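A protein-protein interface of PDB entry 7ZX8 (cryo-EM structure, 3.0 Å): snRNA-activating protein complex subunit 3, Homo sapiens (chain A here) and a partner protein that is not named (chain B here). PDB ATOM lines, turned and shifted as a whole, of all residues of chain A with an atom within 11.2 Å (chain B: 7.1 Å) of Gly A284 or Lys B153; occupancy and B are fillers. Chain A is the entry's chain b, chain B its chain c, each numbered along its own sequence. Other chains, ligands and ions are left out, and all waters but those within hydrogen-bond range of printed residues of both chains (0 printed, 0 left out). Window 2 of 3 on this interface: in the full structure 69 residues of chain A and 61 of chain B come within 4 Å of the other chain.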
ATOM      1  N   TYR A 253      -7.917 -25.313  13.662  1.00  0.00           N
ATOM      2  CA  TYR A 253      -8.592 -24.518  14.673  1.00  0.00           C
ATOM      3  C   TYR A 253      -8.217 -23.057  14.513  1.00  0.00           C
ATOM      4  O   TYR A 253      -7.039 -22.695  14.641  1.00  0.00           O
ATOM      5  CB  TYR A 253      -8.228 -24.996  16.067  1.00  0.00           C
ATOM      6  CG  TYR A 253      -8.766 -24.098  17.140  1.00  0.00           C
ATOM      7  CD1 TYR A 253     -10.125 -23.936  17.307  1.00  0.00           C
ATOM      8  CD2 TYR A 253      -7.916 -23.402  17.979  1.00  0.00           C
ATOM      9  CE1 TYR A 253     -10.624 -23.122  18.283  1.00  0.00           C
ATOM     10  CE2 TYR A 253      -8.409 -22.577  18.960  1.00  0.00           C
ATOM     11  CZ  TYR A 253      -9.766 -22.440  19.108  1.00  0.00           C
ATOM     12  OH  TYR A 253     -10.271 -21.619  20.083  1.00  0.00           O
ATOM     13  N   GLY A 256     -11.768 -20.025  17.753  1.00  0.00           N
ATOM     14  CA  GLY A 256     -12.930 -20.700  18.290  1.00  0.00           C
ATOM     15  C   GLY A 256     -13.507 -21.723  17.340  1.00  0.00           C
ATOM     16  O   GLY A 256     -13.888 -22.819  17.753  1.00  0.00           O
ATOM     17  N   PHE A 258     -13.773 -24.538  14.393  1.00  0.00           N
ATOM     18  CA  PHE A 258     -13.022 -25.660  13.846  1.00  0.00           C
ATOM     19  C   PHE A 258     -13.354 -25.756  12.366  1.00  0.00           C
ATOM     20  O   PHE A 258     -14.459 -25.400  11.944  1.00  0.00           O
ATOM     21  CB  PHE A 258     -13.366 -26.963  14.561  1.00  0.00           C
ATOM     22  CG  PHE A 258     -12.827 -27.054  15.952  1.00  0.00           C
ATOM     23  CD1 PHE A 258     -11.472 -27.186  16.171  1.00  0.00           C
ATOM     24  CD2 PHE A 258     -13.677 -27.027  17.038  1.00  0.00           C
ATOM     25  CE1 PHE A 258     -10.974 -27.275  17.443  1.00  0.00           C
ATOM     26  CE2 PHE A 258     -13.183 -27.115  18.314  1.00  0.00           C
ATOM     27  CZ  PHE A 258     -11.831 -27.240  18.516  1.00  0.00           C
ATOM     28  N   ILE A 274     -13.194 -32.705  21.112  1.00  0.00           N
ATOM     29  CA  ILE A 274     -12.981 -31.511  21.920  1.00  0.00           C
ATOM     30  C   ILE A 274     -14.309 -30.934  22.379  1.00  0.00           C
ATOM     31  O   ILE A 274     -14.514 -30.698  23.578  1.00  0.00           O
ATOM     32  CB  ILE A 274     -12.155 -30.473  21.143  1.00  0.00           C
ATOM     33  CG1 ILE A 274     -10.721 -30.964  20.951  1.00  0.00           C
ATOM     34  CG2 ILE A 274     -12.166 -29.151  21.873  1.00  0.00           C
ATOM     35  CD1 ILE A 274     -10.496 -31.739  19.683  1.00  0.00           C
ATOM     36  N   ILE A 275     -15.246 -30.741  21.448  1.00  0.00           N
ATOM     37  CA  ILE A 275     -16.549 -30.195  21.812  1.00  0.00           C
ATOM     38  C   ILE A 275     -17.153 -30.990  22.956  1.00  0.00           C
ATOM     39  O   ILE A 275     -17.769 -30.426  23.867  1.00  0.00           O
ATOM     40  CB  ILE A 275     -17.483 -30.183  20.592  1.00  0.00           C
ATOM     41  CG1 ILE A 275     -16.768 -29.590  19.381  1.00  0.00           C
ATOM     42  CG2 ILE A 275     -18.737 -29.391  20.905  1.00  0.00           C
ATOM     43  CD1 ILE A 275     -16.332 -28.171  19.582  1.00  0.00           C
ATOM     44  N   GLU A 276     -16.947 -32.311  22.944  1.00  0.00           N
ATOM     45  CA  GLU A 276     -17.571 -33.186  23.932  1.00  0.00           C
ATOM     46  C   GLU A 276     -17.251 -32.744  25.353  1.00  0.00           C
ATOM     47  O   GLU A 276     -18.093 -32.848  26.250  1.00  0.00           O
ATOM     48  CB  GLU A 276     -17.128 -34.626  23.703  1.00  0.00           C
ATOM     49  CG  GLU A 276     -17.385 -35.125  22.295  1.00  0.00           C
ATOM     50  CD  GLU A 276     -18.856 -35.097  21.927  1.00  0.00           C
ATOM     51  OE1 GLU A 276     -19.341 -34.041  21.464  1.00  0.00           O
ATOM     52  OE2 GLU A 276     -19.528 -36.132  22.103  1.00  0.00           O
ATOM     53  N   TRP A 277     -16.043 -32.241  25.583  1.00  0.00           N
ATOM     54  CA  TRP A 277     -15.758 -31.810  26.942  1.00  0.00           C
ATOM     55  C   TRP A 277     -15.710 -30.302  27.092  1.00  0.00           C
ATOM     56  O   TRP A 277     -15.400 -29.818  28.184  1.00  0.00           O
ATOM     57  CB  TRP A 277     -14.459 -32.422  27.448  1.00  0.00           C
ATOM     58  CG  TRP A 277     -13.274 -32.075  26.662  1.00  0.00           C
ATOM     59  CD1 TRP A 277     -12.756 -32.780  25.635  1.00  0.00           C
ATOM     60  CD2 TRP A 277     -12.417 -30.946  26.857  1.00  0.00           C
ATOM     61  NE1 TRP A 277     -11.632 -32.162  25.158  1.00  0.00           N
ATOM     62  CE2 TRP A 277     -11.399 -31.035  25.898  1.00  0.00           C
ATOM     63  CE3 TRP A 277     -12.412 -29.869  27.745  1.00  0.00           C
ATOM     64  CZ2 TRP A 277     -10.388 -30.085  25.793  1.00  0.00           C
ATOM     65  CZ3 TRP A 277     -11.409 -28.930  27.642  1.00  0.00           C
ATOM     66  CH2 TRP A 277     -10.413 -29.042  26.674  1.00  0.00           C
ATOM     67  N   SER A 278     -16.016 -29.548  26.046  1.00  0.00           N
ATOM     68  CA  SER A 278     -16.202 -28.122  26.249  1.00  0.00           C
ATOM     69  C   SER A 278     -17.656 -27.815  26.578  1.00  0.00           C
ATOM     70  O   SER A 278     -17.964 -26.770  27.159  1.00  0.00           O
ATOM     71  CB  SER A 278     -15.743 -27.346  25.018  1.00  0.00           C
ATOM     72  OG  SER A 278     -14.341 -27.158  25.052  1.00  0.00           O
ATOM     73  N   GLU A 279     -18.563 -28.718  26.208  1.00  0.00           N
ATOM     74  CA  GLU A 279     -19.960 -28.559  26.591  1.00  0.00           C
ATOM     75  C   GLU A 279     -20.186 -29.016  28.025  1.00  0.00           C
ATOM     76  O   GLU A 279     -20.930 -28.382  28.782  1.00  0.00           O
ATOM     77  CB  GLU A 279     -20.862 -29.324  25.620  1.00  0.00           C
ATOM     78  CG  GLU A 279     -20.497 -30.788  25.440  1.00  0.00           C
ATOM     79  CD  GLU A 279     -21.021 -31.365  24.139  1.00  0.00           C
ATOM     80  OE1 GLU A 279     -22.127 -31.943  24.147  1.00  0.00           O
ATOM     81  OE2 GLU A 279     -20.326 -31.243  23.106  1.00  0.00           O
ATOM     82  N   SER A 280     -19.552 -30.117  28.418  1.00  0.00           N
ATOM     83  CA  SER A 280     -19.703 -30.690  29.747  1.00  0.00           C
ATOM     84  C   SER A 280     -18.414 -30.496  30.530  1.00  0.00           C
ATOM     85  O   SER A 280     -17.323 -30.767  30.017  1.00  0.00           O
ATOM     86  CB  SER A 280     -20.041 -32.175  29.671  1.00  0.00           C
ATOM     87  OG  SER A 280     -19.088 -32.860  28.883  1.00  0.00           O
ATOM     88  N   HIS A 281     -18.551 -30.042  31.774  1.00  0.00           N
ATOM     89  CA  HIS A 281     -17.400 -29.703  32.602  1.00  0.00           C
ATOM     90  C   HIS A 281     -16.535 -28.668  31.903  1.00  0.00           C
ATOM     91  O   HIS A 281     -15.421 -28.976  31.475  1.00  0.00           O
ATOM     92  CB  HIS A 281     -16.569 -30.939  32.952  1.00  0.00           C
ATOM     93  CG  HIS A 281     -16.966 -31.582  34.241  1.00  0.00           C
ATOM     94  ND1 HIS A 281     -17.815 -32.665  34.306  1.00  0.00           N
ATOM     95  CD2 HIS A 281     -16.647 -31.277  35.521  1.00  0.00           C
ATOM     96  CE1 HIS A 281     -17.991 -33.009  35.566  1.00  0.00           C
ATOM     97  NE2 HIS A 281     -17.292 -32.183  36.324  1.00  0.00           N
ATOM     98  N   ASP A 282     -17.070 -27.459  31.735  1.00  0.00           N
ATOM     99  CA  ASP A 282     -16.324 -26.359  31.140  1.00  0.00           C
ATOM    100  C   ASP A 282     -14.961 -26.213  31.795  1.00  0.00           C
ATOM    101  O   ASP A 282     -14.867 -25.899  32.985  1.00  0.00           O
ATOM    102  CB  ASP A 282     -17.112 -25.053  31.264  1.00  0.00           C
ATOM    103  CG  ASP A 282     -16.420 -23.880  30.590  1.00  0.00           C
ATOM    104  OD1 ASP A 282     -17.031 -23.275  29.688  1.00  0.00           O
ATOM    105  OD2 ASP A 282     -15.278 -23.543  30.971  1.00  0.00           O
ATOM    106  N   ARG A 283     -13.903 -26.430  31.026  1.00  0.00           N
ATOM    107  CA  ARG A 283     -12.538 -26.210  31.484  1.00  0.00           C
ATOM    108  C   ARG A 283     -11.925 -25.137  30.595  1.00  0.00           C
ATOM    109  O   ARG A 283     -11.207 -25.438  29.639  1.00  0.00           O
ATOM    110  CB  ARG A 283     -11.746 -27.521  31.444  1.00  0.00           C
ATOM    111  CG  ARG A 283     -12.422 -28.636  32.235  1.00  0.00           C
ATOM    112  CD  ARG A 283     -11.689 -29.969  32.174  1.00  0.00           C
ATOM    113  NE  ARG A 283     -11.511 -30.470  30.816  1.00  0.00           N
ATOM    114  CZ  ARG A 283     -11.204 -31.732  30.529  1.00  0.00           C
ATOM    115  NH1 ARG A 283     -11.062 -32.613  31.504  1.00  0.00           N
ATOM    116  NH2 ARG A 283     -11.046 -32.114  29.272  1.00  0.00           N
ATOM    117  N   GLY A 284     -12.193 -23.877  30.937  1.00  0.00           N
ATOM    118  CA  GLY A 284     -11.878 -22.763  30.069  1.00  0.00           C
ATOM    119  C   GLY A 284     -12.578 -22.852  28.726  1.00  0.00           C
ATOM    120  O   GLY A 284     -13.499 -23.656  28.551  1.00  0.00           O
ATOM    121  N   TYR A 285     -12.191 -21.983  27.793  1.00  0.00           N
ATOM    122  CA  TYR A 285     -12.486 -22.137  26.371  1.00  0.00           C
ATOM    123  C   TYR A 285     -13.942 -21.888  26.002  1.00  0.00           C
ATOM    124  O   TYR A 285     -14.277 -21.865  24.816  1.00  0.00           O
ATOM    125  CB  TYR A 285     -12.068 -23.529  25.897  1.00  0.00           C
ATOM    126  CG  TYR A 285     -10.592 -23.645  25.655  1.00  0.00           C
ATOM    127  CD1 TYR A 285      -9.946 -22.770  24.801  1.00  0.00           C
ATOM    128  CD2 TYR A 285      -9.844 -24.622  26.278  1.00  0.00           C
ATOM    129  CE1 TYR A 285      -8.596 -22.867  24.574  1.00  0.00           C
ATOM    130  CE2 TYR A 285      -8.492 -24.728  26.054  1.00  0.00           C
ATOM    131  CZ  TYR A 285      -7.874 -23.850  25.203  1.00  0.00           C
ATOM    132  OH  TYR A 285      -6.524 -23.947  24.976  1.00  0.00           O
ATOM    133  N   GLY A 286     -14.805 -21.688  26.995  1.00  0.00           N
ATOM    134  CA  GLY A 286     -16.187 -21.289  26.770  1.00  0.00           C
ATOM    135  C   GLY A 286     -16.910 -21.995  25.629  1.00  0.00           C
ATOM    136  O   GLY A 286     -17.074 -23.215  25.597  1.00  0.00           O
ATOM    137  N   LYS A 287     -17.356 -21.178  24.685  1.00  0.00           N
ATOM    138  CA  LYS A 287     -18.173 -21.596  23.543  1.00  0.00           C
ATOM    139  C   LYS A 287     -17.257 -22.101  22.425  1.00  0.00           C
ATOM    140  O   LYS A 287     -16.071 -21.761  22.378  1.00  0.00           O
ATOM    141  CB  LYS A 287     -19.074 -20.434  23.156  1.00  0.00           C
ATOM    142  CG  LYS A 287     -20.084 -20.714  22.050  1.00  0.00           C
ATOM    143  CD  LYS A 287     -20.740 -22.075  22.195  1.00  0.00           C
ATOM    144  CE  LYS A 287     -21.544 -22.418  20.952  1.00  0.00           C
ATOM    145  NZ  LYS A 287     -21.841 -23.872  20.868  1.00  0.00           N
ATOM    146  N   PHE A 288     -17.795 -22.908  21.508  1.00  0.00           N
ATOM    147  CA  PHE A 288     -17.036 -23.443  20.383  1.00  0.00           C
ATOM    148  C   PHE A 288     -17.901 -23.536  19.137  1.00  0.00           C
ATOM    149  O   PHE A 288     -19.131 -23.575  19.234  1.00  0.00           O
ATOM    150  CB  PHE A 288     -16.474 -24.817  20.726  1.00  0.00           C
ATOM    151  CG  PHE A 288     -15.065 -24.789  21.218  1.00  0.00           C
ATOM    152  CD1 PHE A 288     -14.029 -24.491  20.363  1.00  0.00           C
ATOM    153  CD2 PHE A 288     -14.776 -25.059  22.537  1.00  0.00           C
ATOM    154  CE1 PHE A 288     -12.734 -24.458  20.813  1.00  0.00           C
ATOM    155  CE2 PHE A 288     -13.484 -25.028  22.991  1.00  0.00           C
ATOM    156  CZ  PHE A 288     -12.462 -24.730  22.129  1.00  0.00           C
ATOM    157  N   PHE A 307      -0.725 -14.943  16.306  1.00  0.00           N
ATOM    158  CA  PHE A 307      -1.431 -15.640  17.370  1.00  0.00           C
ATOM    159  C   PHE A 307      -1.564 -17.110  17.002  1.00  0.00           C
ATOM    160  O   PHE A 307      -1.993 -17.432  15.887  1.00  0.00           O
ATOM    161  CB  PHE A 307      -2.803 -15.018  17.608  1.00  0.00           C
ATOM    162  CG  PHE A 307      -3.541 -15.617  18.759  1.00  0.00           C
ATOM    163  CD1 PHE A 307      -3.153 -15.345  20.057  1.00  0.00           C
ATOM    164  CD2 PHE A 307      -4.623 -16.446  18.549  1.00  0.00           C
ATOM    165  CE1 PHE A 307      -3.831 -15.888  21.122  1.00  0.00           C
ATOM    166  CE2 PHE A 307      -5.305 -16.993  19.612  1.00  0.00           C
ATOM    167  CZ  PHE A 307      -4.908 -16.715  20.903  1.00  0.00           C
ATOM    168  N   PHE B 145       1.143 -23.858  23.892  1.00  0.00           N
ATOM    169  CA  PHE B 145       0.373 -24.333  22.754  1.00  0.00           C
ATOM    170  C   PHE B 145       1.102 -25.463  22.047  1.00  0.00           C
ATOM    171  O   PHE B 145       1.021 -25.596  20.824  1.00  0.00           O
ATOM    172  CB  PHE B 145       0.091 -23.188  21.785  1.00  0.00           C
ATOM    173  CG  PHE B 145      -0.560 -22.002  22.424  1.00  0.00           C
ATOM    174  CD1 PHE B 145      -1.933 -21.922  22.529  1.00  0.00           C
ATOM    175  CD2 PHE B 145       0.200 -20.965  22.918  1.00  0.00           C
ATOM    176  CE1 PHE B 145      -2.531 -20.831  23.112  1.00  0.00           C
ATOM    177  CE2 PHE B 145      -0.393 -19.873  23.501  1.00  0.00           C
ATOM    178  CZ  PHE B 145      -1.761 -19.807  23.600  1.00  0.00           C
ATOM    179  N   TYR B 149      -2.518 -28.872  22.805  1.00  0.00           N
ATOM    180  CA  TYR B 149      -2.842 -27.486  22.481  1.00  0.00           C
ATOM    181  C   TYR B 149      -4.043 -26.997  23.276  1.00  0.00           C
ATOM    182  O   TYR B 149      -4.156 -25.802  23.566  1.00  0.00           O
ATOM    183  CB  TYR B 149      -3.093 -27.338  20.985  1.00  0.00           C
ATOM    184  CG  TYR B 149      -3.557 -25.958  20.579  1.00  0.00           C
ATOM    185  CD1 TYR B 149      -2.648 -24.952  20.310  1.00  0.00           C
ATOM    186  CD2 TYR B 149      -4.906 -25.664  20.472  1.00  0.00           C
ATOM    187  CE1 TYR B 149      -3.071 -23.698  19.944  1.00  0.00           C
ATOM    188  CE2 TYR B 149      -5.332 -24.412  20.109  1.00  0.00           C
ATOM    189  CZ  TYR B 149      -4.412 -23.435  19.848  1.00  0.00           C
ATOM    190  OH  TYR B 149      -4.843 -22.185  19.485  1.00  0.00           O
ATOM    191  N   PHE B 150      -4.953 -27.896  23.630  1.00  0.00           N
ATOM    192  CA  PHE B 150      -6.140 -27.526  24.395  1.00  0.00           C
ATOM    193  C   PHE B 150      -5.944 -27.945  25.843  1.00  0.00           C
ATOM    194  O   PHE B 150      -6.416 -29.004  26.263  1.00  0.00           O
ATOM    195  CB  PHE B 150      -7.378 -28.175  23.806  1.00  0.00           C
ATOM    196  CG  PHE B 150      -7.873 -27.512  22.569  1.00  0.00           C
ATOM    197  CD1 PHE B 150      -8.841 -26.534  22.642  1.00  0.00           C
ATOM    198  CD2 PHE B 150      -7.385 -27.875  21.336  1.00  0.00           C
ATOM    199  CE1 PHE B 150      -9.306 -25.927  21.506  1.00  0.00           C
ATOM    200  CE2 PHE B 150      -7.847 -27.274  20.197  1.00  0.00           C
ATOM    201  CZ  PHE B 150      -8.809 -26.296  20.281  1.00  0.00           C
ATOM    202  N   LYS B 151      -5.261 -27.116  26.620  1.00  0.00           N
ATOM    203  CA  LYS B 151      -5.077 -27.395  28.035  1.00  0.00           C
ATOM    204  C   LYS B 151      -6.248 -26.819  28.815  1.00  0.00           C
ATOM    205  O   LYS B 151      -6.852 -25.829  28.394  1.00  0.00           O
ATOM    206  CB  LYS B 151      -3.753 -26.815  28.514  1.00  0.00           C
ATOM    207  CG  LYS B 151      -2.558 -27.426  27.825  1.00  0.00           C
ATOM    208  CD  LYS B 151      -1.256 -26.780  28.237  1.00  0.00           C
ATOM    209  CE  LYS B 151      -0.111 -27.334  27.414  1.00  0.00           C
ATOM    210  NZ  LYS B 151       1.192 -26.734  27.792  1.00  0.00           N
ATOM    211  N   ASP B 152      -6.572 -27.433  29.944  1.00  0.00           N
ATOM    212  CA  ASP B 152      -7.671 -26.966  30.769  1.00  0.00           C
ATOM    213  C   ASP B 152      -7.217 -25.834  31.678  1.00  0.00           C
ATOM    214  O   ASP B 152      -6.023 -25.588  31.854  1.00  0.00           O
ATOM    215  CB  ASP B 152      -8.222 -28.106  31.616  1.00  0.00           C
ATOM    216  CG  ASP B 152      -8.648 -29.284  30.782  1.00  0.00           C
ATOM    217  OD1 ASP B 152      -9.007 -29.076  29.606  1.00  0.00           O
ATOM    218  OD2 ASP B 152      -8.618 -30.419  31.298  1.00  0.00           O
ATOM    219  N   LYS B 153      -8.191 -25.133  32.258  1.00  0.00           N
ATOM    220  CA  LYS B 153      -7.897 -24.104  33.242  1.00  0.00           C
ATOM    221  C   LYS B 153      -8.051 -24.581  34.675  1.00  0.00           C
ATOM    222  O   LYS B 153      -7.320 -24.104  35.545  1.00  0.00           O
ATOM    223  CB  LYS B 153      -8.791 -22.877  33.023  1.00  0.00           C
ATOM    224  CG  LYS B 153      -8.127 -21.779  32.208  1.00  0.00           C
ATOM    225  CD  LYS B 153      -8.007 -22.169  30.741  1.00  0.00           C
ATOM    226  CE  LYS B 153      -6.915 -21.380  30.036  1.00  0.00           C
ATOM    227  NZ  LYS B 153      -6.638 -21.916  28.677  1.00  0.00           N
ATOM    228  N   VAL B 154      -8.969 -25.507  34.940  1.00  0.00           N
ATOM    229  CA  VAL B 154      -9.066 -26.119  36.256  1.00  0.00           C
ATOM    230  C   VAL B 154      -8.027 -27.216  36.453  1.00  0.00           C
ATOM    231  O   VAL B 154      -7.725 -27.565  37.605  1.00  0.00           O
ATOM    232  CB  VAL B 154     -10.481 -26.677  36.508  1.00  0.00           C
ATOM    233  CG1 VAL B 154     -11.505 -25.560  36.459  1.00  0.00           C
ATOM    234  CG2 VAL B 154     -10.818 -27.758  35.490  1.00  0.00           C
ATOM    235  N   THR B 155      -7.474 -27.762  35.377  1.00  0.00           N
ATOM    236  CA  THR B 155      -6.431 -28.776  35.457  1.00  0.00           C
ATOM    237  C   THR B 155      -5.348 -28.384  34.460  1.00  0.00           C
ATOM    238  O   THR B 155      -5.357 -27.281  33.901  1.00  0.00           O
ATOM    239  CB  THR B 155      -6.983 -30.183  35.175  1.00  0.00           C
ATOM    240  OG1 THR B 155      -7.163 -30.348  33.765  1.00  0.00           O
ATOM    241  CG2 THR B 155      -8.306 -30.416  35.888  1.00  0.00           C
ATOM    242  N   GLY B 156      -4.403 -29.288  34.223  1.00  0.00           N
ATOM    243  CA  GLY B 156      -3.358 -29.044  33.252  1.00  0.00           C
ATOM    244  C   GLY B 156      -3.397 -30.042  32.116  1.00  0.00           C
ATOM    245  O   GLY B 156      -2.657 -29.917  31.138  1.00  0.00           O
ATOM    246  N   VAL B 157      -4.267 -31.041  32.240  1.00  0.00           N
ATOM    247  CA  VAL B 157      -4.361 -32.086  31.232  1.00  0.00           C
ATOM    248  C   VAL B 157      -5.136 -31.561  30.034  1.00  0.00           C
ATOM    249  O   VAL B 157      -5.933 -30.620  30.148  1.00  0.00           O
ATOM    250  CB  VAL B 157      -5.025 -33.339  31.830  1.00  0.00           C
ATOM    251  CG1 VAL B 157      -6.488 -33.074  32.127  1.00  0.00           C
ATOM    252  CG2 VAL B 157      -4.854 -34.540  30.913  1.00  0.00           C
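OD2 of Asp B152 is in salt-bridge range of NE of Arg A283, 2.9 Å away.
The side-chain hydroxyl of Tyr A285 lies within hydrogen-bond range of the backbone carbonyl oxygen of Tyr B149 (3.3 Å).
The side-chain hydroxyl of Tyr A253 is in hydrogen-bond range of the backbone NH of Gly A256, 3.2 Å away.
N of Gly A284 lies within hydrogen-bond range of OD2 of Asp A282 (3.1 Å).
OD2 of Asp B152 is in hydrogen-bond range of OG1 of Thr B155 (2.9 Å).
N of Asp B152 lies close to O of Val B157 (3.3 Å).
Among the printed residues, merely in contact across the chains: Tyr A253 with Tyr B149 (3.5 Å), Tyr A253 with Phe B150 (3.8 Å), Phe A258 with Phe B150 (3.6 Å), Trp A277 with Asp B152 (3.1 Å), Arg A283 with Val B154 (3.7 Å), Gly A284 with Lys B153 (3.97 Å), Tyr A285 with Phe B150 (3.6 Å), Tyr A285 with Lys B151 (3.1 Å) and Phe A288 with Phe B150 (3.4 Å).
Of the printed residues of chain B, Tyr A253 touches Tyr B149 and Phe B150.
Of the printed residues of chain B, Trp A277 touches Asp B152.
Ser A280 touches none of the printed residues of chain B.
Of chain B, only Lys B153 (3.97 Å) comes within 4 Å of Gly A284.
Of the printed residues of chain A, Tyr B149 touches Tyr A253 and Tyr A285.
Of the printed residues of chain A, Phe B150 touches Tyr A253 (3.8 Å), Phe A258 (3.6 Å), Tyr A285 (3.6 Å) and Phe A288 (3.4 Å).
Val B154 touches one residue of chain A.
No residue of chain A comes within 4 Å of Thr B155.
The nearest printed residue of chain B that does not touch Gly A284 is Val B154 (5.4 Å).
Among the printed residues, 11 pairs touch across the chains.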
